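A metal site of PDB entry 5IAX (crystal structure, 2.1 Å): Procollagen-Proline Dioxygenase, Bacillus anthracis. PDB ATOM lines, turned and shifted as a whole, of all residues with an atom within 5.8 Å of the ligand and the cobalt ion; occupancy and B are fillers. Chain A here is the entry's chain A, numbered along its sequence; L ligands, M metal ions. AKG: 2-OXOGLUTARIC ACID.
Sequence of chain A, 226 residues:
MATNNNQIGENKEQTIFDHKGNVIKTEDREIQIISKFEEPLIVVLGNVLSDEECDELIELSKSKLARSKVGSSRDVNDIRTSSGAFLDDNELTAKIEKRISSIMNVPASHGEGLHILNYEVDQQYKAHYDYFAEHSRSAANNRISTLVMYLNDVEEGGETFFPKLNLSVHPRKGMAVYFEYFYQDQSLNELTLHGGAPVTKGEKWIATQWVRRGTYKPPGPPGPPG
The indole nitrogen of Trp 210 lies close to an oxygen (O1) of the ligand, at 3.1 Å.
The side-chain hydroxyl of Thr 160 is in hydrogen-bond range of an oxygen (O3) of the ligand (2.6 Å).
OG1 of Thr 208 sits at hydrogen-bond distance from O2 of the ligand, 2.9 Å away.
The side-chain amino group (NZ) of Lys 204 lies within salt-bridge range of an oxygen (O3) of the ligand, 2.7 Å away.
OH of Tyr 119 is in hydrogen-bond range of O4 of the ligand (2.6 Å).
O1 of the ligand binds the cobalt ion (2.0 Å).
NE2 of His 194 binds the cobalt ion (2.0 Å).
The cobalt ion is bound by OD1 of Asp 130, 2.1 Å away.
O5 of the ligand binds the cobalt ion (2.1 Å).
The cobalt ion is bound by NE2 of His 128, 2.1 Å away.
Merely in contact with the ligand: Tyr 125 (3.8 Å), Gly 196 (3.7 Å) and Ile 206 (3.4 Å).
Hydrophobic or aromatic side chains within 4 Å of the ligand: Tyr 119, Tyr 125, His 128, His 194, Ile 206 and Trp 210.
The nearest printed residue that does not touch the ligand is Val 148 (4.03 Å).
NZ of Lys 204 lies within hydrogen-bond range of O of Gly 158.
The backbone NH of Tyr 119 sits at hydrogen-bond distance from the backbone carbonyl oxygen of Lys 204 (2.7 Å).
The backbone NH (N) of Thr 208 sits at hydrogen-bond distance from the backbone carbonyl oxygen (O) of His 115, at 2.7 Å.
OD2 of Asp 130 is in hydrogen-bond range of OG1 of Thr 146 (2.7 Å).
The side-chain hydroxyl (OG1) of Thr 160 sits at hydrogen-bond distance from the side-chain hydroxyl (OH) of Tyr 150.
The backbone carbonyl oxygen (O) of Ile 206 lies within hydrogen-bond range of the backbone NH (N) of Leu 117 (2.9 Å).
N of Tyr 125 lies within hydrogen-bond range of O of Gly 196, 2.8 Å away.
OD2 of Asp 130 sits at hydrogen-bond distance from NE1 of Trp 210 (3.2 Å).
Within 4 Å of the cobalt ion: His 128, Asp 130 and His 194.
Along chain A the residues within 4 Å of the cobalt ion span positions 128 to 194.
The nearest printed residue that does not touch the cobalt ion is Tyr 125 (4.4 Å).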
ATOM      1  N   HIS A 115      16.964  15.160  24.206  1.00  0.00           N
ATOM      2  CA  HIS A 115      17.820  13.997  24.403  1.00  0.00           C
ATOM      3  C   HIS A 115      19.263  14.477  24.549  1.00  0.00           C
ATOM      4  O   HIS A 115      19.798  15.144  23.646  1.00  0.00           O
ATOM      5  CB  HIS A 115      17.670  13.006  23.240  1.00  0.00           C
ATOM      6  CG  HIS A 115      18.471  11.754  23.396  1.00  0.00           C
ATOM      7  ND1 HIS A 115      19.745  11.614  22.870  1.00  0.00           N
ATOM      8  CD2 HIS A 115      18.215  10.590  24.053  1.00  0.00           C
ATOM      9  CE1 HIS A 115      20.223  10.424  23.183  1.00  0.00           C
ATOM     10  NE2 HIS A 115      19.312   9.779  23.906  1.00  0.00           N
ATOM     11  N   LEU A 117      23.335  13.717  25.138  1.00  0.00           N
ATOM     12  CA  LEU A 117      24.332  12.697  24.820  1.00  0.00           C
ATOM     13  C   LEU A 117      25.727  13.231  25.081  1.00  0.00           C
ATOM     14  O   LEU A 117      26.050  14.370  24.719  1.00  0.00           O
ATOM     15  CB  LEU A 117      24.226  12.246  23.350  1.00  0.00           C
ATOM     16  CG  LEU A 117      25.225  11.211  22.857  1.00  0.00           C
ATOM     17  CD1 LEU A 117      25.321  10.030  23.829  1.00  0.00           C
ATOM     18  CD2 LEU A 117      24.737  10.726  21.508  1.00  0.00           C
ATOM     19  N   TYR A 119      29.870  12.331  24.661  1.00  0.00           N
ATOM     20  CA  TYR A 119      30.951  11.531  24.088  1.00  0.00           C
ATOM     21  C   TYR A 119      32.221  11.804  24.874  1.00  0.00           C
ATOM     22  O   TYR A 119      32.663  12.961  24.941  1.00  0.00           O
ATOM     23  CB  TYR A 119      31.231  11.869  22.623  1.00  0.00           C
ATOM     24  CG  TYR A 119      30.065  11.808  21.684  1.00  0.00           C
ATOM     25  CD1 TYR A 119      29.166  12.870  21.590  1.00  0.00           C
ATOM     26  CD2 TYR A 119      29.896  10.731  20.846  1.00  0.00           C
ATOM     27  CE1 TYR A 119      28.095  12.824  20.703  1.00  0.00           C
ATOM     28  CE2 TYR A 119      28.837  10.658  19.964  1.00  0.00           C
ATOM     29  CZ  TYR A 119      27.958  11.719  19.880  1.00  0.00           C
ATOM     30  OH  TYR A 119      26.925  11.626  18.985  1.00  0.00           O
ATOM     31  N   TYR A 125      29.467   8.486  16.919  1.00  0.00           N
ATOM     32  CA  TYR A 125      28.148   8.012  16.517  1.00  0.00           C
ATOM     33  C   TYR A 125      28.242   7.629  15.049  1.00  0.00           C
ATOM     34  O   TYR A 125      28.322   8.495  14.170  1.00  0.00           O
ATOM     35  CB  TYR A 125      27.109   9.114  16.783  1.00  0.00           C
ATOM     36  CG  TYR A 125      25.645   8.697  16.829  1.00  0.00           C
ATOM     37  CD1 TYR A 125      25.209   7.474  16.300  1.00  0.00           C
ATOM     38  CD2 TYR A 125      24.679   9.552  17.361  1.00  0.00           C
ATOM     39  CE1 TYR A 125      23.843   7.092  16.322  1.00  0.00           C
ATOM     40  CE2 TYR A 125      23.317   9.183  17.385  1.00  0.00           C
ATOM     41  CZ  TYR A 125      22.911   7.957  16.867  1.00  0.00           C
ATOM     42  OH  TYR A 125      21.579   7.617  16.891  1.00  0.00           O
ATOM     43  N   HIS A 128      24.209   7.186  10.309  1.00  0.00           N
ATOM     44  CA  HIS A 128      22.901   6.563  10.459  1.00  0.00           C
ATOM     45  C   HIS A 128      21.892   7.511   9.866  1.00  0.00           C
ATOM     46  O   HIS A 128      22.214   8.654   9.526  1.00  0.00           O
ATOM     47  CB  HIS A 128      22.572   6.299  11.926  1.00  0.00           C
ATOM     48  CG  HIS A 128      22.623   7.533  12.754  1.00  0.00           C
ATOM     49  ND1 HIS A 128      23.791   8.011  13.306  1.00  0.00           N
ATOM     50  CD2 HIS A 128      21.660   8.451  13.042  1.00  0.00           C
ATOM     51  CE1 HIS A 128      23.542   9.161  13.922  1.00  0.00           C
ATOM     52  NE2 HIS A 128      22.261   9.431  13.787  1.00  0.00           N
ATOM     53  N   TYR A 129      20.673   7.013   9.743  1.00  0.00           N
ATOM     54  CA  TYR A 129      19.539   7.864   9.444  1.00  0.00           C
ATOM     55  C   TYR A 129      18.791   8.121  10.737  1.00  0.00           C
ATOM     56  O   TYR A 129      18.685   7.224  11.580  1.00  0.00           O
ATOM     57  CB  TYR A 129      18.619   7.215   8.415  1.00  0.00           C
ATOM     58  CG  TYR A 129      19.276   6.951   7.064  1.00  0.00           C
ATOM     59  CD1 TYR A 129      19.610   7.999   6.210  1.00  0.00           C
ATOM     60  CD2 TYR A 129      19.539   5.643   6.647  1.00  0.00           C
ATOM     61  CE1 TYR A 129      20.221   7.759   4.971  1.00  0.00           C
ATOM     62  CE2 TYR A 129      20.156   5.392   5.415  1.00  0.00           C
ATOM     63  CZ  TYR A 129      20.484   6.461   4.583  1.00  0.00           C
ATOM     64  OH  TYR A 129      21.072   6.224   3.370  1.00  0.00           O
ATOM     65  N   ASP A 130      18.264   9.347  10.912  1.00  0.00           N
ATOM     66  CA  ASP A 130      17.465   9.575  12.108  1.00  0.00           C
ATOM     67  C   ASP A 130      16.045   9.036  11.965  1.00  0.00           C
ATOM     68  O   ASP A 130      15.431   8.688  12.970  1.00  0.00           O
ATOM     69  CB  ASP A 130      17.408  11.054  12.476  1.00  0.00           C
ATOM     70  CG  ASP A 130      18.645  11.505  13.201  1.00  0.00           C
ATOM     71  OD1 ASP A 130      19.485  10.627  13.505  1.00  0.00           O
ATOM     72  OD2 ASP A 130      18.785  12.730  13.442  1.00  0.00           O
ATOM     73  N   THR A 146      15.417  17.097  12.566  1.00  0.00           N
ATOM     74  CA  THR A 146      16.318  16.914  13.687  1.00  0.00           C
ATOM     75  C   THR A 146      16.951  18.252  13.985  1.00  0.00           C
ATOM     76  O   THR A 146      17.236  19.019  13.066  1.00  0.00           O
ATOM     77  CB  THR A 146      17.439  15.883  13.349  1.00  0.00           C
ATOM     78  OG1 THR A 146      16.886  14.591  13.033  1.00  0.00           O
ATOM     79  CG2 THR A 146      18.402  15.736  14.499  1.00  0.00           C
ATOM     80  N   VAL A 148      20.389  19.276  16.266  1.00  0.00           N
ATOM     81  CA  VAL A 148      21.511  18.912  17.144  1.00  0.00           C
ATOM     82  C   VAL A 148      22.130  20.188  17.698  1.00  0.00           C
ATOM     83  O   VAL A 148      22.712  20.987  16.955  1.00  0.00           O
ATOM     84  CB  VAL A 148      22.579  18.078  16.399  1.00  0.00           C
ATOM     85  CG1 VAL A 148      23.778  17.862  17.285  1.00  0.00           C
ATOM     86  CG2 VAL A 148      22.006  16.770  15.912  1.00  0.00           C
ATOM     87  N   TYR A 150      24.889  21.984  20.239  1.00  0.00           N
ATOM     88  CA  TYR A 150      26.206  21.739  20.822  1.00  0.00           C
ATOM     89  C   TYR A 150      26.258  22.418  22.183  1.00  0.00           C
ATOM     90  O   TYR A 150      26.204  23.645  22.275  1.00  0.00           O
ATOM     91  CB  TYR A 150      27.296  22.258  19.907  1.00  0.00           C
ATOM     92  CG  TYR A 150      27.260  21.632  18.555  1.00  0.00           C
ATOM     93  CD1 TYR A 150      27.499  20.266  18.393  1.00  0.00           C
ATOM     94  CD2 TYR A 150      26.994  22.390  17.425  1.00  0.00           C
ATOM     95  CE1 TYR A 150      27.454  19.678  17.138  1.00  0.00           C
ATOM     96  CE2 TYR A 150      26.955  21.818  16.158  1.00  0.00           C
ATOM     97  CZ  TYR A 150      27.202  20.452  16.019  1.00  0.00           C
ATOM     98  OH  TYR A 150      27.156  19.894  14.768  1.00  0.00           O
ATOM     99  N   GLY A 158      34.705  15.343  16.833  1.00  0.00           N
ATOM    100  CA  GLY A 158      33.311  15.522  17.210  1.00  0.00           C
ATOM    101  C   GLY A 158      32.415  16.229  16.207  1.00  0.00           C
ATOM    102  O   GLY A 158      31.321  16.656  16.580  1.00  0.00           O
ATOM    103  N   GLU A 159      32.819  16.325  14.938  1.00  0.00           N
ATOM    104  CA  GLU A 159      31.983  17.032  13.965  1.00  0.00           C
ATOM    105  C   GLU A 159      30.779  16.193  13.577  1.00  0.00           C
ATOM    106  O   GLU A 159      30.821  14.950  13.561  1.00  0.00           O
ATOM    107  CB  GLU A 159      32.777  17.435  12.712  1.00  0.00           C
ATOM    108  CG  GLU A 159      33.686  16.419  12.130  1.00  0.00           C
ATOM    109  CD  GLU A 159      35.065  16.463  12.794  1.00  0.00           C
ATOM    110  OE1 GLU A 159      35.254  15.828  13.820  1.00  0.00           O
ATOM    111  OE2 GLU A 159      35.954  17.191  12.324  1.00  0.00           O
ATOM    112  N   THR A 160      29.685  16.879  13.306  1.00  0.00           N
ATOM    113  CA  THR A 160      28.522  16.235  12.711  1.00  0.00           C
ATOM    114  C   THR A 160      28.794  16.176  11.223  1.00  0.00           C
ATOM    115  O   THR A 160      28.967  17.219  10.589  1.00  0.00           O
ATOM    116  CB  THR A 160      27.237  17.028  12.980  1.00  0.00           C
ATOM    117  OG1 THR A 160      27.106  17.301  14.372  1.00  0.00           O
ATOM    118  CG2 THR A 160      26.026  16.263  12.478  1.00  0.00           C
ATOM    119  N   PHE A 161      28.907  14.977  10.647  1.00  0.00           N
ATOM    120  CA  PHE A 161      29.300  14.866   9.256  1.00  0.00           C
ATOM    121  C   PHE A 161      28.234  14.135   8.477  1.00  0.00           C
ATOM    122  O   PHE A 161      27.584  13.210   8.985  1.00  0.00           O
ATOM    123  CB  PHE A 161      30.661  14.146   9.086  1.00  0.00           C
ATOM    124  CG  PHE A 161      30.615  12.708   9.529  1.00  0.00           C
ATOM    125  CD1 PHE A 161      30.721  12.382  10.864  1.00  0.00           C
ATOM    126  CD2 PHE A 161      30.413  11.699   8.608  1.00  0.00           C
ATOM    127  CE1 PHE A 161      30.664  11.070  11.293  1.00  0.00           C
ATOM    128  CE2 PHE A 161      30.344  10.353   9.039  1.00  0.00           C
ATOM    129  CZ  PHE A 161      30.469  10.056  10.387  1.00  0.00           C
ATOM    130  N   PHE A 179      18.363  19.821  10.212  1.00  0.00           N
ATOM    131  CA  PHE A 179      18.242  19.092   8.957  1.00  0.00           C
ATOM    132  C   PHE A 179      16.887  18.389   8.910  1.00  0.00           C
ATOM    133  O   PHE A 179      16.326  18.052   9.938  1.00  0.00           O
ATOM    134  CB  PHE A 179      19.441  18.182   8.645  1.00  0.00           C
ATOM    135  CG  PHE A 179      19.703  17.113   9.677  1.00  0.00           C
ATOM    136  CD1 PHE A 179      20.402  17.398  10.822  1.00  0.00           C
ATOM    137  CD2 PHE A 179      19.285  15.817   9.459  1.00  0.00           C
ATOM    138  CE1 PHE A 179      20.671  16.419  11.751  1.00  0.00           C
ATOM    139  CE2 PHE A 179      19.541  14.828  10.384  1.00  0.00           C
ATOM    140  CZ  PHE A 179      20.234  15.129  11.530  1.00  0.00           C
ATOM    141  N   HIS A 194      24.127  10.734   8.367  1.00  0.00           N
ATOM    142  CA  HIS A 194      25.028  11.573   9.151  1.00  0.00           C
ATOM    143  C   HIS A 194      25.537  10.817  10.373  1.00  0.00           C
ATOM    144  O   HIS A 194      24.939   9.835  10.817  1.00  0.00           O
ATOM    145  CB  HIS A 194      24.331  12.807   9.662  1.00  0.00           C
ATOM    146  CG  HIS A 194      23.200  12.494  10.583  1.00  0.00           C
ATOM    147  ND1 HIS A 194      21.963  12.096  10.117  1.00  0.00           N
ATOM    148  CD2 HIS A 194      23.120  12.451  11.934  1.00  0.00           C
ATOM    149  CE1 HIS A 194      21.157  11.878  11.140  1.00  0.00           C
ATOM    150  NE2 HIS A 194      21.843  12.081  12.258  1.00  0.00           N
ATOM    151  N   GLY A 195      26.568  11.378  10.982  1.00  0.00           N
ATOM    152  CA  GLY A 195      27.099  10.824  12.204  1.00  0.00           C
ATOM    153  C   GLY A 195      27.897  11.842  12.996  1.00  0.00           C
ATOM    154  O   GLY A 195      28.131  12.976  12.562  1.00  0.00           O
ATOM    155  N   GLY A 196      28.312  11.406  14.174  1.00  0.00           N
ATOM    156  CA  GLY A 196      29.141  12.184  15.047  1.00  0.00           C
ATOM    157  C   GLY A 196      30.517  11.592  15.018  1.00  0.00           C
ATOM    158  O   GLY A 196      30.700  10.426  15.399  1.00  0.00           O
ATOM    159  N   ALA A 197      31.487  12.362  14.507  1.00  0.00           N
ATOM    160  CA  ALA A 197      32.849  11.881  14.339  1.00  0.00           C
ATOM    161  C   ALA A 197      33.528  11.672  15.691  1.00  0.00           C
ATOM    162  O   ALA A 197      33.196  12.344  16.673  1.00  0.00           O
ATOM    163  CB  ALA A 197      33.669  12.871  13.503  1.00  0.00           C
ATOM    164  N   LYS A 204      32.399  15.768  24.333  1.00  0.00           N
ATOM    165  CA  LYS A 204      31.348  16.428  23.568  1.00  0.00           C
ATOM    166  C   LYS A 204      30.009  16.175  24.236  1.00  0.00           C
ATOM    167  O   LYS A 204      29.643  15.030  24.484  1.00  0.00           O
ATOM    168  CB  LYS A 204      31.324  15.911  22.123  1.00  0.00           C
ATOM    169  CG  LYS A 204      30.143  16.394  21.266  1.00  0.00           C
ATOM    170  CD  LYS A 204      30.362  15.974  19.797  1.00  0.00           C
ATOM    171  CE  LYS A 204      29.058  15.896  19.023  1.00  0.00           C
ATOM    172  NZ  LYS A 204      29.230  15.329  17.665  1.00  0.00           N
ATOM    173  N   ILE A 206      25.863  17.104  23.658  1.00  0.00           N
ATOM    174  CA  ILE A 206      24.835  17.588  22.744  1.00  0.00           C
ATOM    175  C   ILE A 206      23.460  17.360  23.324  1.00  0.00           C
ATOM    176  O   ILE A 206      23.228  16.465  24.156  1.00  0.00           O
ATOM    177  CB  ILE A 206      24.884  16.916  21.341  1.00  0.00           C
ATOM    178  CG1 ILE A 206      24.751  15.391  21.437  1.00  0.00           C
ATOM    179  CG2 ILE A 206      26.147  17.381  20.530  1.00  0.00           C
ATOM    180  CD1 ILE A 206      24.546  14.687  20.050  1.00  0.00           C
ATOM    181  N   THR A 208      19.697  16.698  21.418  1.00  0.00           N
ATOM    182  CA  THR A 208      19.019  16.472  20.154  1.00  0.00           C
ATOM    183  C   THR A 208      17.509  16.559  20.351  1.00  0.00           C
ATOM    184  O   THR A 208      16.954  16.016  21.304  1.00  0.00           O
ATOM    185  CB  THR A 208      19.417  15.132  19.557  1.00  0.00           C
ATOM    186  OG1 THR A 208      20.838  15.073  19.487  1.00  0.00           O
ATOM    187  CG2 THR A 208      18.872  14.982  18.149  1.00  0.00           C
ATOM    188  N   TRP A 210      14.440  15.308  18.188  1.00  0.00           N
ATOM    189  CA  TRP A 210      13.884  14.633  17.021  1.00  0.00           C
ATOM    190  C   TRP A 210      12.395  14.963  16.943  1.00  0.00           C
ATOM    191  O   TRP A 210      11.684  14.876  17.946  1.00  0.00           O
ATOM    192  CB  TRP A 210      14.104  13.118  17.104  1.00  0.00           C
ATOM    193  CG  TRP A 210      15.567  12.712  17.104  1.00  0.00           C
ATOM    194  CD1 TRP A 210      16.435  12.824  16.076  1.00  0.00           C
ATOM    195  CD2 TRP A 210      16.294  12.101  18.196  1.00  0.00           C
ATOM    196  NE1 TRP A 210      17.665  12.334  16.449  1.00  0.00           N
ATOM    197  CE2 TRP A 210      17.613  11.890  17.739  1.00  0.00           C
ATOM    198  CE3 TRP A 210      15.959  11.701  19.501  1.00  0.00           C
ATOM    199  CZ2 TRP A 210      18.621  11.310  18.551  1.00  0.00           C
ATOM    200  CZ3 TRP A 210      16.944  11.113  20.309  1.00  0.00           C
ATOM    201  CH2 TRP A 210      18.262  10.929  19.834  1.00  0.00           C
HETATM  202  C1  AKG L   1      21.649  12.575  16.455  1.00  0.00           C
HETATM  203  O1  AKG L   1      20.700  12.119  15.785  1.00  0.00           O
HETATM  204  O2  AKG L   1      21.499  12.982  17.616  1.00  0.00           O
HETATM  205  C2  AKG L   1      23.017  12.673  15.857  1.00  0.00           C
HETATM  206  O5  AKG L   1      23.200  12.181  14.827  1.00  0.00           O
HETATM  207  C3  AKG L   1      24.106  13.411  16.641  1.00  0.00           C
HETATM  208  C4  AKG L   1      25.288  13.727  15.749  1.00  0.00           C
HETATM  209  C5  AKG L   1      26.448  14.323  16.540  1.00  0.00           C
HETATM  210  O3  AKG L   1      27.070  15.308  16.078  1.00  0.00           O
HETATM  211  O4  AKG L   1      26.787  13.860  17.659  1.00  0.00           O
HETATM  212 CO    CO M   1      21.369  11.353  14.113  1.00  0.00          CO
